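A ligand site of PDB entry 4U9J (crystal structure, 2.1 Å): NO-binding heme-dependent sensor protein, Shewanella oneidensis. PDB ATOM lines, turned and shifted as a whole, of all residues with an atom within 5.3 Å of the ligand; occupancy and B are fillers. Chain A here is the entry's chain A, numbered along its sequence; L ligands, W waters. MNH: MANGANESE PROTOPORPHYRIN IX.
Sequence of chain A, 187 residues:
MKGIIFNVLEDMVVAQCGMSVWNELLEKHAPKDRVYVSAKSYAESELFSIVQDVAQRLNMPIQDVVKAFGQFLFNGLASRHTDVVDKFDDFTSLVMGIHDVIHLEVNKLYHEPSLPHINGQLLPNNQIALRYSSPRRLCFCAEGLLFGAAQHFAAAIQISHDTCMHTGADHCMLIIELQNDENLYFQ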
ATOM      1  N   MET A   1       7.438  23.195 -19.613  1.00  0.00           N
ATOM      2  CA  MET A   1       7.478  22.630 -18.212  1.00  0.00           C
ATOM      3  C   MET A   1       6.233  21.799 -17.943  1.00  0.00           C
ATOM      4  O   MET A   1       5.092  22.294 -18.024  1.00  0.00           O
ATOM      5  CB  MET A   1       7.598  23.781 -17.209  1.00  0.00           C
ATOM      6  CG  MET A   1       7.861  23.392 -15.761  1.00  0.00           C
ATOM      7  SD  MET A   1       9.494  22.763 -15.559  1.00  0.00           S
ATOM      8  CE  MET A   1      10.535  24.245 -15.836  1.00  0.00           C
ATOM      9  N   LYS A   2       6.439  20.506 -17.675  1.00  0.00           N
ATOM     10  CA  LYS A   2       5.300  19.579 -17.496  1.00  0.00           C
ATOM     11  C   LYS A   2       4.541  19.857 -16.226  1.00  0.00           C
ATOM     12  O   LYS A   2       5.096  20.238 -15.186  1.00  0.00           O
ATOM     13  CB  LYS A   2       5.795  18.119 -17.517  1.00  0.00           C
ATOM     14  CG  LYS A   2       6.288  17.655 -18.916  1.00  0.00           C
ATOM     15  CD  LYS A   2       5.235  17.792 -19.973  1.00  0.00           C
ATOM     16  CE  LYS A   2       5.680  17.179 -21.232  1.00  0.00           C
ATOM     17  NZ  LYS A   2       4.644  17.309 -22.299  1.00  0.00           N
ATOM     18  N   ILE A   4       3.432  17.952 -14.110  1.00  0.00           N
ATOM     19  CA  ILE A   4       3.843  17.239 -12.936  1.00  0.00           C
ATOM     20  C   ILE A   4       4.789  18.079 -12.062  1.00  0.00           C
ATOM     21  O   ILE A   4       4.696  17.994 -10.825  1.00  0.00           O
ATOM     22  CB  ILE A   4       4.540  15.937 -13.257  1.00  0.00           C
ATOM     23  CG1 ILE A   4       4.987  15.267 -11.952  1.00  0.00           C
ATOM     24  CG2 ILE A   4       5.718  16.149 -14.161  1.00  0.00           C
ATOM     25  CD1 ILE A   4       5.071  13.874 -12.041  1.00  0.00           C
ATOM     26  N   ILE A   5       5.620  18.926 -12.673  1.00  0.00           N
ATOM     27  CA  ILE A   5       6.500  19.759 -11.882  1.00  0.00           C
ATOM     28  C   ILE A   5       5.670  20.766 -11.040  1.00  0.00           C
ATOM     29  O   ILE A   5       5.937  20.984  -9.840  1.00  0.00           O
ATOM     30  CB  ILE A   5       7.508  20.510 -12.746  1.00  0.00           C
ATOM     31  CG1 ILE A   5       8.260  19.522 -13.624  1.00  0.00           C
ATOM     32  CG2 ILE A   5       8.449  21.366 -11.870  1.00  0.00           C
ATOM     33  CD1 ILE A   5       8.973  18.391 -12.919  1.00  0.00           C
ATOM     34  N   PHE A  74      12.379  15.346  -5.754  1.00  0.00           N
ATOM     35  CA  PHE A  74      12.843  14.019  -6.013  1.00  0.00           C
ATOM     36  C   PHE A  74      11.811  13.054  -5.492  1.00  0.00           C
ATOM     37  O   PHE A  74      11.495  12.093  -6.170  1.00  0.00           O
ATOM     38  CB  PHE A  74      14.202  13.661  -5.404  1.00  0.00           C
ATOM     39  CG  PHE A  74      14.643  12.276  -5.784  1.00  0.00           C
ATOM     40  CD1 PHE A  74      14.254  11.156  -5.043  1.00  0.00           C
ATOM     41  CD2 PHE A  74      15.338  12.083  -6.949  1.00  0.00           C
ATOM     42  CE1 PHE A  74      14.585   9.869  -5.445  1.00  0.00           C
ATOM     43  CE2 PHE A  74      15.699  10.799  -7.345  1.00  0.00           C
ATOM     44  CZ  PHE A  74      15.323   9.690  -6.589  1.00  0.00           C
ATOM     45  N   LEU A  77       8.694  12.984  -7.719  1.00  0.00           N
ATOM     46  CA  LEU A  77       8.904  12.236  -8.931  1.00  0.00           C
ATOM     47  C   LEU A  77       9.017  10.740  -8.621  1.00  0.00           C
ATOM     48  O   LEU A  77       8.367   9.919  -9.329  1.00  0.00           O
ATOM     49  CB  LEU A  77      10.138  12.729  -9.684  1.00  0.00           C
ATOM     50  CG  LEU A  77      10.072  14.149 -10.290  1.00  0.00           C
ATOM     51  CD1 LEU A  77      11.470  14.624 -10.744  1.00  0.00           C
ATOM     52  CD2 LEU A  77       9.092  14.241 -11.440  1.00  0.00           C
ATOM     53  N   ALA A  78       9.737  10.366  -7.569  1.00  0.00           N
ATOM     54  CA  ALA A  78       9.915   8.946  -7.265  1.00  0.00           C
ATOM     55  C   ALA A  78       8.601   8.331  -6.886  1.00  0.00           C
ATOM     56  O   ALA A  78       8.377   7.178  -7.147  1.00  0.00           O
ATOM     57  CB  ALA A  78      10.922   8.689  -6.164  1.00  0.00           C
ATOM     58  N   HIS A  81       6.548   7.982 -10.246  1.00  0.00           N
ATOM     59  CA  HIS A  81       7.246   7.125 -11.217  1.00  0.00           C
ATOM     60  C   HIS A  81       8.116   6.108 -10.512  1.00  0.00           C
ATOM     61  O   HIS A  81       9.324   5.969 -10.735  1.00  0.00           O
ATOM     62  CB  HIS A  81       8.132   7.944 -12.183  1.00  0.00           C
ATOM     63  CG  HIS A  81       7.376   8.873 -13.090  1.00  0.00           C
ATOM     64  ND1 HIS A  81       6.567   8.431 -14.100  1.00  0.00           N
ATOM     65  CD2 HIS A  81       7.326  10.215 -13.136  1.00  0.00           C
ATOM     66  CE1 HIS A  81       6.044   9.463 -14.735  1.00  0.00           C
ATOM     67  NE2 HIS A  81       6.475  10.558 -14.179  1.00  0.00           N
ATOM     68  N   VAL A  84      10.409   3.709 -12.385  1.00  0.00           N
ATOM     69  CA  VAL A  84      11.673   4.233 -12.886  1.00  0.00           C
ATOM     70  C   VAL A  84      12.767   4.230 -11.789  1.00  0.00           C
ATOM     71  O   VAL A  84      13.873   3.710 -11.991  1.00  0.00           O
ATOM     72  CB  VAL A  84      11.465   5.654 -13.482  1.00  0.00           C
ATOM     73  CG1 VAL A  84      12.740   6.215 -13.911  1.00  0.00           C
ATOM     74  CG2 VAL A  84      10.490   5.531 -14.708  1.00  0.00           C
ATOM     75  N   VAL A  85      12.436   4.707 -10.599  1.00  0.00           N
ATOM     76  CA  VAL A  85      13.409   4.780  -9.484  1.00  0.00           C
ATOM     77  C   VAL A  85      13.772   3.383  -8.974  1.00  0.00           C
ATOM     78  O   VAL A  85      14.896   3.168  -8.578  1.00  0.00           O
ATOM     79  CB  VAL A  85      12.886   5.628  -8.363  1.00  0.00           C
ATOM     80  CG1 VAL A  85      13.894   5.749  -7.264  1.00  0.00           C
ATOM     81  CG2 VAL A  85      12.716   7.090  -8.905  1.00  0.00           C
ATOM     82  N   LEU A  94      21.805   5.307  -9.696  1.00  0.00           N
ATOM     83  CA  LEU A  94      20.795   6.219 -10.138  1.00  0.00           C
ATOM     84  C   LEU A  94      21.423   7.427 -10.808  1.00  0.00           C
ATOM     85  O   LEU A  94      20.995   7.820 -11.883  1.00  0.00           O
ATOM     86  CB  LEU A  94      19.898   6.674  -8.988  1.00  0.00           C
ATOM     87  CG  LEU A  94      18.687   7.532  -9.438  1.00  0.00           C
ATOM     88  CD1 LEU A  94      17.478   7.238  -8.592  1.00  0.00           C
ATOM     89  CD2 LEU A  94      18.999   9.065  -9.422  1.00  0.00           C
ATOM     90  N   VAL A  95      22.444   8.033 -10.184  1.00  0.00           N
ATOM     91  CA  VAL A  95      23.029   9.223 -10.752  1.00  0.00           C
ATOM     92  C   VAL A  95      23.660   8.914 -12.128  1.00  0.00           C
ATOM     93  O   VAL A  95      23.474   9.668 -13.082  1.00  0.00           O
ATOM     94  CB  VAL A  95      24.072   9.866  -9.794  1.00  0.00           C
ATOM     95  CG1 VAL A  95      24.802  11.038 -10.537  1.00  0.00           C
ATOM     96  CG2 VAL A  95      23.395  10.353  -8.507  1.00  0.00           C
ATOM     97  N   ILE A  98      20.856   8.803 -14.868  1.00  0.00           N
ATOM     98  CA  ILE A  98      19.877   9.890 -15.008  1.00  0.00           C
ATOM     99  C   ILE A  98      19.624  10.131 -16.487  1.00  0.00           C
ATOM    100  O   ILE A  98      18.498  10.188 -16.904  1.00  0.00           O
ATOM    101  CB  ILE A  98      20.333  11.179 -14.376  1.00  0.00           C
ATOM    102  CG1 ILE A  98      20.300  11.067 -12.863  1.00  0.00           C
ATOM    103  CG2 ILE A  98      19.415  12.366 -14.846  1.00  0.00           C
ATOM    104  CD1 ILE A  98      21.241  12.107 -12.188  1.00  0.00           C
ATOM    105  N   ILE A 102      16.815   7.141 -16.757  1.00  0.00           N
ATOM    106  CA  ILE A 102      15.680   7.908 -16.259  1.00  0.00           C
ATOM    107  C   ILE A 102      15.080   8.834 -17.333  1.00  0.00           C
ATOM    108  O   ILE A 102      13.903   8.777 -17.598  1.00  0.00           O
ATOM    109  CB  ILE A 102      16.062   8.729 -15.018  1.00  0.00           C
ATOM    110  CG1 ILE A 102      16.523   7.820 -13.859  1.00  0.00           C
ATOM    111  CG2 ILE A 102      14.916   9.574 -14.588  1.00  0.00           C
ATOM    112  CD1 ILE A 102      16.890   8.546 -12.642  1.00  0.00           C
ATOM    113  N   HIS A 103      15.884   9.656 -17.991  1.00  0.00           N
ATOM    114  CA  HIS A 103      15.364  10.685 -18.819  1.00  0.00           C
ATOM    115  C   HIS A 103      15.054  10.032 -20.194  1.00  0.00           C
ATOM    116  O   HIS A 103      14.211  10.507 -20.946  1.00  0.00           O
ATOM    117  CB  HIS A 103      16.344  11.900 -18.882  1.00  0.00           C
ATOM    118  CG  HIS A 103      16.283  12.826 -17.685  1.00  0.00           C
ATOM    119  ND1 HIS A 103      17.253  13.769 -17.403  1.00  0.00           N
ATOM    120  CD2 HIS A 103      15.345  12.964 -16.718  1.00  0.00           C
ATOM    121  CE1 HIS A 103      16.906  14.445 -16.309  1.00  0.00           C
ATOM    122  NE2 HIS A 103      15.759  13.962 -15.844  1.00  0.00           N
ATOM    123  N   VAL A 106      11.556   9.104 -19.414  1.00  0.00           N
ATOM    124  CA  VAL A 106      10.733  10.310 -19.397  1.00  0.00           C
ATOM    125  C   VAL A 106      10.352  10.720 -20.830  1.00  0.00           C
ATOM    126  O   VAL A 106       9.192  11.093 -21.065  1.00  0.00           O
ATOM    127  CB  VAL A 106      11.451  11.467 -18.617  1.00  0.00           C
ATOM    128  CG1 VAL A 106      10.693  12.770 -18.680  1.00  0.00           C
ATOM    129  CG2 VAL A 106      11.642  11.067 -17.177  1.00  0.00           C
ATOM    130  N   TYR A 110       6.269  10.942 -21.569  1.00  0.00           N
ATOM    131  CA  TYR A 110       5.734  12.264 -21.807  1.00  0.00           C
ATOM    132  C   TYR A 110       5.974  12.650 -23.262  1.00  0.00           C
ATOM    133  O   TYR A 110       6.974  12.310 -23.835  1.00  0.00           O
ATOM    134  CB  TYR A 110       6.374  13.331 -20.912  1.00  0.00           C
ATOM    135  CG  TYR A 110       6.144  13.172 -19.427  1.00  0.00           C
ATOM    136  CD1 TYR A 110       6.950  12.381 -18.669  1.00  0.00           C
ATOM    137  CD2 TYR A 110       5.080  13.811 -18.789  1.00  0.00           C
ATOM    138  CE1 TYR A 110       6.713  12.194 -17.278  1.00  0.00           C
ATOM    139  CE2 TYR A 110       4.837  13.634 -17.415  1.00  0.00           C
ATOM    140  CZ  TYR A 110       5.663  12.826 -16.675  1.00  0.00           C
ATOM    141  OH  TYR A 110       5.441  12.622 -15.327  1.00  0.00           O
ATOM    142  N   GLU A 112       7.373  15.054 -25.735  1.00  0.00           N
ATOM    143  CA  GLU A 112       8.351  16.158 -25.888  1.00  0.00           C
ATOM    144  C   GLU A 112       8.643  16.905 -24.605  1.00  0.00           C
ATOM    145  O   GLU A 112       8.454  18.093 -24.535  1.00  0.00           O
ATOM    146  CB  GLU A 112       7.877  17.151 -26.984  1.00  0.00           C
ATOM    147  CG  GLU A 112       7.911  16.468 -28.382  1.00  0.00           C
ATOM    148  CD  GLU A 112       7.392  17.333 -29.527  1.00  0.00           C
ATOM    149  OE1 GLU A 112       7.031  18.525 -29.295  1.00  0.00           O
ATOM    150  OE2 GLU A 112       7.269  16.832 -30.694  1.00  0.00           O
ATOM    151  N   PRO A 113       9.141  16.196 -23.597  1.00  0.00           N
ATOM    152  CA  PRO A 113       9.535  16.888 -22.375  1.00  0.00           C
ATOM    153  C   PRO A 113      10.780  17.775 -22.680  1.00  0.00           C
ATOM    154  O   PRO A 113      11.445  17.547 -23.669  1.00  0.00           O
ATOM    155  CB  PRO A 113       9.848  15.731 -21.415  1.00  0.00           C
ATOM    156  CG  PRO A 113      10.462  14.722 -22.324  1.00  0.00           C
ATOM    157  CD  PRO A 113       9.646  14.819 -23.615  1.00  0.00           C
ATOM    158  N   SER A 114      11.017  18.758 -21.821  1.00  0.00           N
ATOM    159  CA  SER A 114      12.154  19.655 -21.906  1.00  0.00           C
ATOM    160  C   SER A 114      13.118  19.388 -20.746  1.00  0.00           C
ATOM    161  O   SER A 114      12.937  19.794 -19.569  1.00  0.00           O
ATOM    162  CB  SER A 114      11.653  21.102 -21.905  1.00  0.00           C
ATOM    163  OG  SER A 114      11.101  21.479 -23.151  1.00  0.00           O
ATOM    164  N   LEU A 115      14.130  18.630 -21.109  1.00  0.00           N
ATOM    165  CA  LEU A 115      14.999  17.980 -20.159  1.00  0.00           C
ATOM    166  C   LEU A 115      16.429  18.502 -20.288  1.00  0.00           C
ATOM    167  O   LEU A 115      16.835  18.904 -21.383  1.00  0.00           O
ATOM    168  CB  LEU A 115      14.998  16.480 -20.396  1.00  0.00           C
ATOM    169  CG  LEU A 115      13.720  15.702 -20.054  1.00  0.00           C
ATOM    170  CD1 LEU A 115      13.714  14.298 -20.627  1.00  0.00           C
ATOM    171  CD2 LEU A 115      13.642  15.681 -18.614  1.00  0.00           C
ATOM    172  N   PRO A 116      17.211  18.469 -19.195  1.00  0.00           N
ATOM    173  CA  PRO A 116      18.607  18.907 -19.346  1.00  0.00           C
ATOM    174  C   PRO A 116      19.441  17.855 -20.069  1.00  0.00           C
ATOM    175  O   PRO A 116      19.045  16.699 -20.185  1.00  0.00           O
ATOM    176  CB  PRO A 116      19.091  19.061 -17.909  1.00  0.00           C
ATOM    177  CG  PRO A 116      18.396  17.932 -17.198  1.00  0.00           C
ATOM    178  CD  PRO A 116      16.978  17.890 -17.865  1.00  0.00           C
ATOM    179  N   ILE A 118      22.787  15.705 -19.378  1.00  0.00           N
ATOM    180  CA  ILE A 118      23.534  15.257 -18.234  1.00  0.00           C
ATOM    181  C   ILE A 118      24.489  14.146 -18.621  1.00  0.00           C
ATOM    182  O   ILE A 118      24.184  13.272 -19.418  1.00  0.00           O
ATOM    183  CB  ILE A 118      22.591  14.815 -17.100  1.00  0.00           C
ATOM    184  CG1 ILE A 118      21.914  16.079 -16.560  1.00  0.00           C
ATOM    185  CG2 ILE A 118      23.391  14.151 -15.909  1.00  0.00           C
ATOM    186  CD1 ILE A 118      20.957  15.852 -15.449  1.00  0.00           C
ATOM    187  N   LEU A 130      29.290  15.119 -12.258  1.00  0.00           N
ATOM    188  CA  LEU A 130      28.089  15.244 -13.044  1.00  0.00           C
ATOM    189  C   LEU A 130      28.060  16.562 -13.848  1.00  0.00           C
ATOM    190  O   LEU A 130      27.991  17.631 -13.282  1.00  0.00           O
ATOM    191  CB  LEU A 130      26.884  15.143 -12.116  1.00  0.00           C
ATOM    192  CG  LEU A 130      25.559  14.835 -12.822  1.00  0.00           C
ATOM    193  CD1 LEU A 130      25.579  13.418 -13.323  1.00  0.00           C
ATOM    194  CD2 LEU A 130      24.337  14.936 -11.911  1.00  0.00           C
ATOM    195  N   TYR A 132      26.157  19.122 -16.229  1.00  0.00           N
ATOM    196  CA  TYR A 132      24.772  19.537 -16.474  1.00  0.00           C
ATOM    197  C   TYR A 132      24.793  20.690 -17.472  1.00  0.00           C
ATOM    198  O   TYR A 132      25.599  21.604 -17.359  1.00  0.00           O
ATOM    199  CB  TYR A 132      24.133  20.005 -15.175  1.00  0.00           C
ATOM    200  CG  TYR A 132      22.833  20.730 -15.320  1.00  0.00           C
ATOM    201  CD1 TYR A 132      22.792  22.106 -15.535  1.00  0.00           C
ATOM    202  CD2 TYR A 132      21.623  20.076 -15.231  1.00  0.00           C
ATOM    203  CE1 TYR A 132      21.567  22.765 -15.677  1.00  0.00           C
ATOM    204  CE2 TYR A 132      20.414  20.744 -15.333  1.00  0.00           C
ATOM    205  CZ  TYR A 132      20.384  22.077 -15.582  1.00  0.00           C
ATOM    206  OH  TYR A 132      19.181  22.772 -15.693  1.00  0.00           O
ATOM    207  N   SER A 134      21.709  23.060 -19.716  1.00  0.00           N
ATOM    208  CA  SER A 134      20.304  23.297 -20.079  1.00  0.00           C
ATOM    209  C   SER A 134      20.062  24.777 -20.306  1.00  0.00           C
ATOM    210  O   SER A 134      20.549  25.585 -19.552  1.00  0.00           O
ATOM    211  CB  SER A 134      19.367  22.827 -18.979  1.00  0.00           C
ATOM    212  OG  SER A 134      18.037  23.313 -19.180  1.00  0.00           O
ATOM    213  N   PRO A 135      19.230  25.143 -21.314  1.00  0.00           N
ATOM    214  CA  PRO A 135      18.958  26.577 -21.538  1.00  0.00           C
ATOM    215  C   PRO A 135      18.092  27.140 -20.387  1.00  0.00           C
ATOM    216  O   PRO A 135      17.934  28.329 -20.225  1.00  0.00           O
ATOM    217  CB  PRO A 135      18.208  26.575 -22.880  1.00  0.00           C
ATOM    218  CG  PRO A 135      17.470  25.196 -22.823  1.00  0.00           C
ATOM    219  CD  PRO A 135      18.466  24.281 -22.240  1.00  0.00           C
ATOM    220  N   ARG A 136      17.544  26.270 -19.583  1.00  0.00           N
ATOM    221  CA  ARG A 136      16.754  26.712 -18.453  1.00  0.00           C
ATOM    222  C   ARG A 136      17.618  26.999 -17.190  1.00  0.00           C
ATOM    223  O   ARG A 136      17.127  27.547 -16.226  1.00  0.00           O
ATOM    224  CB  ARG A 136      15.702  25.657 -18.128  1.00  0.00           C
ATOM    225  CG  ARG A 136      14.592  25.605 -19.195  1.00  0.00           C
ATOM    226  CD  ARG A 136      13.787  24.295 -19.130  1.00  0.00           C
ATOM    227  NE  ARG A 136      14.580  23.157 -19.583  1.00  0.00           N
ATOM    228  CZ  ARG A 136      14.838  22.896 -20.850  1.00  0.00           C
ATOM    229  NH1 ARG A 136      14.342  23.669 -21.776  1.00  0.00           N
ATOM    230  NH2 ARG A 136      15.554  21.844 -21.180  1.00  0.00           N
ATOM    231  N   LEU A 138      18.733  25.356 -14.588  1.00  0.00           N
ATOM    232  CA  LEU A 138      18.135  24.884 -13.338  1.00  0.00           C
ATOM    233  C   LEU A 138      19.108  23.964 -12.548  1.00  0.00           C
ATOM    234  O   LEU A 138      18.688  22.957 -11.972  1.00  0.00           O
ATOM    235  CB  LEU A 138      16.815  24.166 -13.649  1.00  0.00           C
ATOM    236  CG  LEU A 138      15.649  25.123 -13.930  1.00  0.00           C
ATOM    237  CD1 LEU A 138      14.398  24.385 -14.518  1.00  0.00           C
ATOM    238  CD2 LEU A 138      15.262  25.832 -12.598  1.00  0.00           C
ATOM    239  N   CYS A 141      18.154  23.325  -9.083  1.00  0.00           N
ATOM    240  CA  CYS A 141      17.125  22.305  -9.006  1.00  0.00           C
ATOM    241  C   CYS A 141      17.799  20.948  -9.066  1.00  0.00           C
ATOM    242  O   CYS A 141      17.428  20.085  -8.342  1.00  0.00           O
ATOM    243  CB  CYS A 141      16.081  22.417 -10.133  1.00  0.00           C
ATOM    244  SG  CYS A 141      14.669  21.348  -9.861  1.00  0.00           S
ATOM    245  N   ALA A 142      18.821  20.796  -9.907  1.00  0.00           N
ATOM    246  CA  ALA A 142      19.545  19.530  -9.983  1.00  0.00           C
ATOM    247  C   ALA A 142      20.268  19.190  -8.705  1.00  0.00           C
ATOM    248  O   ALA A 142      20.246  18.006  -8.335  1.00  0.00           O
ATOM    249  CB  ALA A 142      20.541  19.545 -11.116  1.00  0.00           C
ATOM    250  N   LEU A 145      17.706  17.856  -6.399  1.00  0.00           N
ATOM    251  CA  LEU A 145      17.249  16.521  -6.822  1.00  0.00           C
ATOM    252  C   LEU A 145      18.265  15.459  -6.373  1.00  0.00           C
ATOM    253  O   LEU A 145      17.857  14.389  -5.959  1.00  0.00           O
ATOM    254  CB  LEU A 145      17.008  16.440  -8.353  1.00  0.00           C
ATOM    255  CG  LEU A 145      15.682  17.033  -8.759  1.00  0.00           C
ATOM    256  CD1 LEU A 145      15.675  17.483 -10.213  1.00  0.00           C
ATOM    257  CD2 LEU A 145      14.585  15.999  -8.581  1.00  0.00           C
ATOM    258  N   LEU A 146      19.557  15.803  -6.390  1.00  0.00           N
ATOM    259  CA  LEU A 146      20.600  14.873  -5.985  1.00  0.00           C
ATOM    260  C   LEU A 146      20.554  14.678  -4.500  1.00  0.00           C
ATOM    261  O   LEU A 146      20.720  13.540  -4.034  1.00  0.00           O
ATOM    262  CB  LEU A 146      21.963  15.372  -6.411  1.00  0.00           C
ATOM    263  CG  LEU A 146      22.162  15.326  -7.913  1.00  0.00           C
ATOM    264  CD1 LEU A 146      23.346  16.187  -8.241  1.00  0.00           C
ATOM    265  CD2 LEU A 146      22.449  13.948  -8.388  1.00  0.00           C
ATOM    266  N   ALA A 149      17.667  12.324  -3.958  1.00  0.00           N
ATOM    267  CA  ALA A 149      18.051  10.981  -4.316  1.00  0.00           C
ATOM    268  C   ALA A 149      18.890  10.382  -3.207  1.00  0.00           C
ATOM    269  O   ALA A 149      18.763   9.201  -2.887  1.00  0.00           O
ATOM    270  CB  ALA A 149      18.843  10.953  -5.613  1.00  0.00           C
HETATM  271 MN   MNH L   1      14.711  14.833 -14.140  1.00  0.00          MN
HETATM  272  CHA MNH L   1      13.321  17.517 -15.342  1.00  0.00           C
HETATM  273  CHB MNH L   1      17.342  16.523 -13.275  1.00  0.00           C
HETATM  274  CHC MNH L   1      15.446  12.583 -11.682  1.00  0.00           C
HETATM  275  CHD MNH L   1      11.820  13.241 -14.444  1.00  0.00           C
HETATM  276  NA  MNH L   1      15.289  16.854 -14.391  1.00  0.00           N
HETATM  277  C1A MNH L   1      14.545  17.898 -14.868  1.00  0.00           C
HETATM  278  C2A MNH L   1      15.253  19.164 -14.639  1.00  0.00           C
HETATM  279  C3A MNH L   1      16.394  18.906 -13.925  1.00  0.00           C
HETATM  280  C4A MNH L   1      16.404  17.438 -13.802  1.00  0.00           C
HETATM  281  CMA MNH L   1      17.486  19.781 -13.340  1.00  0.00           C
HETATM  282  CAA MNH L   1      14.625  20.512 -15.044  1.00  0.00           C
HETATM  283  CBA MNH L   1      14.845  20.958 -16.489  1.00  0.00           C
HETATM  284  CGA MNH L   1      16.196  21.401 -17.000  1.00  0.00           C
HETATM  285  O1A MNH L   1      16.373  21.641 -18.220  1.00  0.00           O
HETATM  286  O2A MNH L   1      17.074  21.444 -16.101  1.00  0.00           O
HETATM  287  NB  MNH L   1      16.413  14.367 -12.861  1.00  0.00           N
HETATM  288  C1B MNH L   1      17.424  15.322 -12.521  1.00  0.00           C
HETATM  289  C2B MNH L   1      18.412  14.887 -11.538  1.00  0.00           C
HETATM  290  C3B MNH L   1      17.738  13.732 -11.219  1.00  0.00           C
HETATM  291  C4B MNH L   1      16.498  13.450 -11.885  1.00  0.00           C
HETATM  292  CMB MNH L   1      19.704  15.641 -11.155  1.00  0.00           C
HETATM  293  CAB MNH L   1      18.156  12.777 -10.179  1.00  0.00           C
HETATM  294  CBB MNH L   1      18.823  12.900  -8.889  1.00  0.00           C
HETATM  295  NC  MNH L   1      13.739  13.109 -13.169  1.00  0.00           N
HETATM  296  C1C MNH L   1      14.214  12.271 -12.155  1.00  0.00           C
HETATM  297  C2C MNH L   1      13.287  11.195 -11.773  1.00  0.00           C
HETATM  298  C3C MNH L   1      12.278  11.452 -12.595  1.00  0.00           C
HETATM  299  C4C MNH L   1      12.528  12.567 -13.457  1.00  0.00           C
HETATM  300  CMC MNH L   1      13.492  10.136 -10.670  1.00  0.00           C
HETATM  301  CAC MNH L   1      11.022  10.680 -12.686  1.00  0.00           C
HETATM  302  CBC MNH L   1      10.962   9.485 -13.461  1.00  0.00           C
HETATM  303  ND  MNH L   1      12.866  15.145 -15.048  1.00  0.00           N
HETATM  304  C1D MNH L   1      11.659  14.466 -15.078  1.00  0.00           C
HETATM  305  C2D MNH L   1      10.522  15.239 -15.675  1.00  0.00           C
HETATM  306  C3D MNH L   1      11.054  16.470 -15.893  1.00  0.00           C
HETATM  307  C4D MNH L   1      12.428  16.458 -15.464  1.00  0.00           C
HETATM  308  CMD MNH L   1       9.169  14.652 -15.883  1.00  0.00           C
HETATM  309  CAD MNH L   1      10.382  17.689 -16.487  1.00  0.00           C
HETATM  310  CBD MNH L   1      10.408  17.732 -18.008  1.00  0.00           C
HETATM  311  CGD MNH L   1       9.592  18.907 -18.546  1.00  0.00           C
HETATM  312  O1D MNH L   1       9.112  19.714 -17.733  1.00  0.00           O
HETATM  313  O2D MNH L   1       9.348  19.075 -19.800  1.00  0.00           O
HETATM  314  O   HOH W   1      11.423  21.744 -18.295  1.00  0.00           O
HETATM  315  O   HOH W   2       7.649  20.701 -20.980  1.00  0.00           O
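Water W2 lies within hydrogen-bond range of O2D of the ligand (2.6 Å) and N of Met 1 (2.9 Å).
Water W1 lies within hydrogen-bond range of O of Ser 114 (2.8 Å), O1D of the ligand (3.1 Å) and SD of Met 1 (3.5 Å).
The backbone NH (N) of His 103 sits at hydrogen-bond distance from the backbone carbonyl oxygen (O) of Ile 98 (2.9 Å).
The side-chain hydroxyl (OH) of Tyr 132 sits at hydrogen-bond distance from the backbone NH (N) of Leu 138.
OG of Ser 134 sits close to N of Arg 136 (3.0 Å).
O of Leu 115 lies within hydrogen-bond range of NH2 of Arg 136.
NE2 of His 81 sits at hydrogen-bond distance from OH of Tyr 110 (2.6 Å).
The side-chain sulfur (SD) of Met 1 lies close to an oxygen (O1D) of the ligand, 3.8 Å away.
The backbone nitrogen of Pro 116 lies close to an oxygen (O1A) of the ligand.
Residues that only touch the ligand: Ile 5, Leu 77, His 81, Val 84, Val 85, Leu 94, Ile 98, Ile 102, Val 106, Tyr 110, Pro 113, Leu 115, Leu 138, Ala 142, Leu 145, Leu 146 and Ala 149.
Hydrophobic or aromatic side chains within 4 Å of the ligand: Met 1, Ile 5, Leu 77, His 81, Val 84, Val 85, Leu 94, Ile 98, Ile 102, His 103, Val 106, Tyr 110, Pro 113, Leu 115, Pro 116, Tyr 132, Leu 138, Ala 142, Leu 145, Leu 146 and Ala 149.
Within 4 Å of the ligand: Met 1, Lys 2, Ile 5, Leu 77, His 81, Val 84, Val 85, Leu 94, Ile 98, Ile 102, His 103, Val 106, Tyr 110, Pro 113, Ser 114, Leu 115, Pro 116, Tyr 132, Ser 134, Arg 136, Leu 138, Ala 142, Leu 145, Leu 146 and Ala 149.
The nearest printed residue that does not touch the ligand is Phe 74 (4.05 Å).
MN of the ligand is bound by NE2 of His 103, at 2.2 Å.
The side-chain hydroxyl of Tyr 132 lies within hydrogen-bond range of an oxygen (O2A) of the ligand (2.5 Å).
The side-chain hydroxyl (OG) of Ser 134 lies within hydrogen-bond range of an oxygen (O1A) of the ligand, 2.5 Å away.
The backbone NH (N) of Ser 114 lies within hydrogen-bond range of an oxygen (O2D) of the ligand (2.6 Å).
An oxygen (O1A) of the ligand is in salt-bridge range of the guanidinium group of Arg 136.
The backbone NH (N) of Lys 2 lies within hydrogen-bond range of an oxygen (O1D) of the ligand (2.8 Å).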
